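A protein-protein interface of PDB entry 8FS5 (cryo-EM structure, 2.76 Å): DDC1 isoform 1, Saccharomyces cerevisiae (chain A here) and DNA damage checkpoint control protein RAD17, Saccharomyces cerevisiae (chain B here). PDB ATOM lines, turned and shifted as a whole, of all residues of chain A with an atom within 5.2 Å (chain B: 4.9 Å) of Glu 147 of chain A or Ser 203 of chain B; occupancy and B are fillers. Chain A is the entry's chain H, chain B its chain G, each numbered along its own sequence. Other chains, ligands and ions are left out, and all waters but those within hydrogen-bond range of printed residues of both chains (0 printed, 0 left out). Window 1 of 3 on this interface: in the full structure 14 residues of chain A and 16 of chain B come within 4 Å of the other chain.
The backbone carbonyl oxygen of Glu 147 of chain A is in hydrogen-bond range of the side-chain hydroxyl of Ser 203 of chain B, at 3.0 Å.
N of Glu 147 of chain A is in hydrogen-bond range of O of Lys 204 of chain B (2.4 Å).
N of Leu 194 of chain B is in hydrogen-bond range of O of Ile 205 of chain B, at 2.9 Å.
The backbone carbonyl oxygen (O) of Ser 203 of chain B lies within hydrogen-bond range of the backbone NH (N) of Ser 196 of chain B (2.7 Å).
Among the printed residues, merely in contact across the chains: Lys 146 of chain A with Lys 204 of chain B, Val 145 of chain A with Ile 205 of chain B, Tyr 148 of chain A with Ser 203 of chain B, Tyr 148 of chain A with Ile 173 of chain B, Cys 149 of chain A with Phe 202 of chain B and Cys 149 of chain A with Gly 201 of chain B.
Ile 135 of chain A touches none of the printed residues of chain B.
Printed residues of chain B within 4 Å of Lys 146 of chain A: Lys 204.
Of chain B, only Ser 203 and Lys 204 come within 4 Å of Glu 147 of chain A.
Printed residues of chain B within 4 Å of Tyr 148 of chain A: Ile 173 and Ser 203.
Of the printed residues of chain B, Cys 149 of chain A touches Gly 201 (3.98 Å) and Phe 202 (3.8 Å).
Of the printed residues of chain A, Ile 173 of chain B touches Tyr 148 (3.6 Å).
Ser 196 of chain B touches none of the printed residues of chain A.
Printed residues of chain A within 4 Å of Phe 202 of chain B: Cys 149 (3.8 Å).
Ser 203 of chain B touches just these residues of chain A: Glu 147 and Tyr 148.
The nearest residue of chain B that does not touch Glu 147 of chain A is Ile 205 of chain B (4.6 Å).
The nearest residue of chain A that does not touch Ser 203 of chain B is Cys 149 of chain A (4.9 Å).
The nearest printed residue of chain B that does not touch Lys 146 of chain A is Ile 205 of chain B (4.3 Å).
Of the 9 printed residues of chain B, 6 touch a printed residue of chain A.
Printed residues of chain B that touch a printed residue of chain A: Ile 173, Gly 201, Phe 202, Ser 203, Lys 204 and Ile 205.
Hydrophobic or aromatic side chains of chain B that line the printed part of chain A: Ile 173.
Of the 8 printed residues of chain A, 5 touch a printed residue of chain B.
Hydrophobic or aromatic side chains of chain A within 4 Å of the printed part of chain B: Tyr 148.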
ATOM      1  N   ILE A 135       1.572 -17.887 -13.105  1.00  0.00           N
ATOM      2  CA  ILE A 135       1.129 -17.242 -11.875  1.00  0.00           C
ATOM      3  C   ILE A 135       1.892 -17.853 -10.710  1.00  0.00           C
ATOM      4  O   ILE A 135       1.791 -19.060 -10.454  1.00  0.00           O
ATOM      5  CB  ILE A 135      -0.388 -17.382 -11.674  1.00  0.00           C
ATOM      6  CG1 ILE A 135      -1.147 -16.549 -12.710  1.00  0.00           C
ATOM      7  CG2 ILE A 135      -0.781 -16.964 -10.266  1.00  0.00           C
ATOM      8  CD1 ILE A 135      -0.513 -15.206 -13.000  1.00  0.00           C
ATOM      9  N   VAL A 136       2.651 -17.025 -10.000  1.00  0.00           N
ATOM     10  CA  VAL A 136       3.385 -17.448  -8.814  1.00  0.00           C
ATOM     11  C   VAL A 136       3.037 -16.491  -7.680  1.00  0.00           C
ATOM     12  O   VAL A 136       3.093 -15.267  -7.853  1.00  0.00           O
ATOM     13  CB  VAL A 136       4.901 -17.500  -9.065  1.00  0.00           C
ATOM     14  CG1 VAL A 136       5.355 -16.309  -9.893  1.00  0.00           C
ATOM     15  CG2 VAL A 136       5.657 -17.573  -7.750  1.00  0.00           C
ATOM     16  N   VAL A 137       2.670 -17.049  -6.528  1.00  0.00           N
ATOM     17  CA  VAL A 137       2.221 -16.278  -5.374  1.00  0.00           C
ATOM     18  C   VAL A 137       3.208 -16.490  -4.235  1.00  0.00           C
ATOM     19  O   VAL A 137       3.526 -17.634  -3.886  1.00  0.00           O
ATOM     20  CB  VAL A 137       0.801 -16.685  -4.944  1.00  0.00           C
ATOM     21  CG1 VAL A 137       0.361 -15.887  -3.724  1.00  0.00           C
ATOM     22  CG2 VAL A 137      -0.178 -16.513  -6.093  1.00  0.00           C
ATOM     23  N   VAL A 145       2.266  -9.784   0.496  1.00  0.00           N
ATOM     24  CA  VAL A 145       1.933 -10.630  -0.643  1.00  0.00           C
ATOM     25  C   VAL A 145       2.609 -10.054  -1.878  1.00  0.00           C
ATOM     26  O   VAL A 145       2.326  -8.919  -2.280  1.00  0.00           O
ATOM     27  CB  VAL A 145       0.413 -10.734  -0.841  1.00  0.00           C
ATOM     28  CG1 VAL A 145       0.097 -11.550  -2.086  1.00  0.00           C
ATOM     29  CG2 VAL A 145      -0.240 -11.349   0.385  1.00  0.00           C
ATOM     30  N   LYS A 146       3.501 -10.834  -2.482  1.00  0.00           N
ATOM     31  CA  LYS A 146       4.221 -10.425  -3.682  1.00  0.00           C
ATOM     32  C   LYS A 146       3.697 -11.223  -4.870  1.00  0.00           C
ATOM     33  O   LYS A 146       3.679 -12.458  -4.834  1.00  0.00           O
ATOM     34  CB  LYS A 146       5.726 -10.624  -3.507  1.00  0.00           C
ATOM     35  CG  LYS A 146       6.245 -10.222  -2.134  1.00  0.00           C
ATOM     36  CD  LYS A 146       7.761 -10.319  -2.044  1.00  0.00           C
ATOM     37  CE  LYS A 146       8.281 -11.615  -2.641  1.00  0.00           C
ATOM     38  NZ  LYS A 146       9.759 -11.732  -2.498  1.00  0.00           N
ATOM     39  N   GLU A 147       3.276 -10.516  -5.914  1.00  0.00           N
ATOM     40  CA  GLU A 147       2.681 -11.117  -7.098  1.00  0.00           C
ATOM     41  C   GLU A 147       3.627 -10.968  -8.281  1.00  0.00           C
ATOM     42  O   GLU A 147       4.239  -9.911  -8.468  1.00  0.00           O
ATOM     43  CB  GLU A 147       1.329 -10.462  -7.427  1.00  0.00           C
ATOM     44  CG  GLU A 147       0.079 -11.322  -7.194  1.00  0.00           C
ATOM     45  CD  GLU A 147       0.147 -12.729  -7.780  1.00  0.00           C
ATOM     46  OE1 GLU A 147      -0.626 -13.588  -7.308  1.00  0.00           O
ATOM     47  OE2 GLU A 147       0.909 -12.974  -8.740  1.00  0.00           O
ATOM     48  N   TYR A 148       3.745 -12.029  -9.073  1.00  0.00           N
ATOM     49  CA  TYR A 148       4.553 -12.020 -10.284  1.00  0.00           C
ATOM     50  C   TYR A 148       3.776 -12.686 -11.410  1.00  0.00           C
ATOM     51  O   TYR A 148       2.985 -13.603 -11.170  1.00  0.00           O
ATOM     52  CB  TYR A 148       5.890 -12.743 -10.084  1.00  0.00           C
ATOM     53  CG  TYR A 148       6.763 -12.161  -8.996  1.00  0.00           C
ATOM     54  CD1 TYR A 148       6.615 -12.556  -7.672  1.00  0.00           C
ATOM     55  CD2 TYR A 148       7.747 -11.227  -9.294  1.00  0.00           C
ATOM     56  CE1 TYR A 148       7.414 -12.030  -6.678  1.00  0.00           C
ATOM     57  CE2 TYR A 148       8.550 -10.696  -8.305  1.00  0.00           C
ATOM     58  CZ  TYR A 148       8.380 -11.102  -6.999  1.00  0.00           C
ATOM     59  OH  TYR A 148       9.177 -10.577  -6.011  1.00  0.00           O
ATOM     60  N   CYS A 149       4.003 -12.222 -12.637  1.00  0.00           N
ATOM     61  CA  CYS A 149       3.364 -12.777 -13.828  1.00  0.00           C
ATOM     62  C   CYS A 149       4.399 -13.058 -14.916  1.00  0.00           C
ATOM     63  O   CYS A 149       4.455 -12.350 -15.929  1.00  0.00           O
ATOM     64  CB  CYS A 149       2.283 -11.830 -14.343  1.00  0.00           C
ATOM     65  SG  CYS A 149       0.754 -11.842 -13.381  1.00  0.00           S
ATOM     66  N   ILE B 173      14.100  -7.301  -9.080  1.00  0.00           N
ATOM     67  CA  ILE B 173      13.329  -7.699 -10.255  1.00  0.00           C
ATOM     68  C   ILE B 173      13.554  -6.708 -11.390  1.00  0.00           C
ATOM     69  O   ILE B 173      12.936  -6.817 -12.454  1.00  0.00           O
ATOM     70  CB  ILE B 173      11.828  -7.837  -9.937  1.00  0.00           C
ATOM     71  CG1 ILE B 173      11.199  -6.462  -9.688  1.00  0.00           C
ATOM     72  CG2 ILE B 173      11.609  -8.791  -8.770  1.00  0.00           C
ATOM     73  CD1 ILE B 173       9.794  -6.521  -9.127  1.00  0.00           C
ATOM     74  N   LEU B 194       2.636  -1.747  -4.644  1.00  0.00           N
ATOM     75  CA  LEU B 194       3.734  -1.173  -5.419  1.00  0.00           C
ATOM     76  C   LEU B 194       3.909  -2.029  -6.671  1.00  0.00           C
ATOM     77  O   LEU B 194       4.697  -2.976  -6.694  1.00  0.00           O
ATOM     78  CB  LEU B 194       5.023  -1.107  -4.580  1.00  0.00           C
ATOM     79  CG  LEU B 194       5.062  -0.054  -3.470  1.00  0.00           C
ATOM     80  CD1 LEU B 194       6.315  -0.207  -2.621  1.00  0.00           C
ATOM     81  CD2 LEU B 194       4.981   1.348  -4.054  1.00  0.00           C
ATOM     82  N   ILE B 195       3.159  -1.686  -7.722  1.00  0.00           N
ATOM     83  CA  ILE B 195       3.194  -2.467  -8.954  1.00  0.00           C
ATOM     84  C   ILE B 195       4.340  -1.989  -9.843  1.00  0.00           C
ATOM     85  O   ILE B 195       4.628  -0.791  -9.953  1.00  0.00           O
ATOM     86  CB  ILE B 195       1.844  -2.392  -9.686  1.00  0.00           C
ATOM     87  CG1 ILE B 195       0.691  -2.676  -8.723  1.00  0.00           C
ATOM     88  CG2 ILE B 195       1.791  -3.389 -10.820  1.00  0.00           C
ATOM     89  CD1 ILE B 195      -0.023  -1.442  -8.237  1.00  0.00           C
ATOM     90  N   SER B 196       5.002  -2.947 -10.494  1.00  0.00           N
ATOM     91  CA  SER B 196       6.234  -2.659 -11.213  1.00  0.00           C
ATOM     92  C   SER B 196       6.172  -3.178 -12.644  1.00  0.00           C
ATOM     93  O   SER B 196       5.600  -4.237 -12.910  1.00  0.00           O
ATOM     94  CB  SER B 196       7.442  -3.276 -10.497  1.00  0.00           C
ATOM     95  OG  SER B 196       8.072  -4.254 -11.307  1.00  0.00           O
ATOM     96  N   GLY B 201       7.624  -9.028 -16.269  1.00  0.00           N
ATOM     97  CA  GLY B 201       6.248  -8.873 -16.686  1.00  0.00           C
ATOM     98  C   GLY B 201       5.576  -7.766 -15.905  1.00  0.00           C
ATOM     99  O   GLY B 201       6.068  -6.634 -15.880  1.00  0.00           O
ATOM    100  N   PHE B 202       4.452  -8.071 -15.263  1.00  0.00           N
ATOM    101  CA  PHE B 202       3.732  -7.082 -14.472  1.00  0.00           C
ATOM    102  C   PHE B 202       3.634  -7.604 -13.042  1.00  0.00           C
ATOM    103  O   PHE B 202       2.738  -8.390 -12.721  1.00  0.00           O
ATOM    104  CB  PHE B 202       2.351  -6.827 -15.067  1.00  0.00           C
ATOM    105  CG  PHE B 202       2.016  -5.373 -15.200  1.00  0.00           C
ATOM    106  CD1 PHE B 202       2.224  -4.497 -14.154  1.00  0.00           C
ATOM    107  CD2 PHE B 202       1.492  -4.881 -16.382  1.00  0.00           C
ATOM    108  CE1 PHE B 202       1.926  -3.158 -14.292  1.00  0.00           C
ATOM    109  CE2 PHE B 202       1.188  -3.543 -16.523  1.00  0.00           C
ATOM    110  CZ  PHE B 202       1.400  -2.681 -15.475  1.00  0.00           C
ATOM    111  N   SER B 203       4.548  -7.163 -12.182  1.00  0.00           N
ATOM    112  CA  SER B 203       4.664  -7.687 -10.830  1.00  0.00           C
ATOM    113  C   SER B 203       4.075  -6.711  -9.819  1.00  0.00           C
ATOM    114  O   SER B 203       4.131  -5.490  -9.990  1.00  0.00           O
ATOM    115  CB  SER B 203       6.128  -7.980 -10.480  1.00  0.00           C
ATOM    116  OG  SER B 203       6.344  -7.893  -9.083  1.00  0.00           O
ATOM    117  N   LYS B 204       3.515  -7.273  -8.749  1.00  0.00           N
ATOM    118  CA  LYS B 204       2.827  -6.498  -7.725  1.00  0.00           C
ATOM    119  C   LYS B 204       3.304  -6.920  -6.343  1.00  0.00           C
ATOM    120  O   LYS B 204       3.428  -8.116  -6.066  1.00  0.00           O
ATOM    121  CB  LYS B 204       1.308  -6.679  -7.828  1.00  0.00           C
ATOM    122  CG  LYS B 204       0.513  -5.837  -6.844  1.00  0.00           C
ATOM    123  CD  LYS B 204      -0.837  -6.468  -6.516  1.00  0.00           C
ATOM    124  CE  LYS B 204      -1.455  -7.161  -7.723  1.00  0.00           C
ATOM    125  NZ  LYS B 204      -2.376  -8.259  -7.324  1.00  0.00           N
ATOM    126  N   ILE B 205       3.564  -5.939  -5.484  1.00  0.00           N
ATOM    127  CA  ILE B 205       3.878  -6.170  -4.077  1.00  0.00           C
ATOM    128  C   ILE B 205       2.776  -5.524  -3.252  1.00  0.00           C
ATOM    129  O   ILE B 205       2.577  -4.305  -3.319  1.00  0.00           O
ATOM    130  CB  ILE B 205       5.253  -5.602  -3.694  1.00  0.00           C
ATOM    131  CG1 ILE B 205       6.347  -6.206  -4.576  1.00  0.00           C
ATOM    132  CG2 ILE B 205       5.543  -5.860  -2.223  1.00  0.00           C
ATOM    133  CD1 ILE B 205       7.744  -5.760  -4.204  1.00  0.00           C
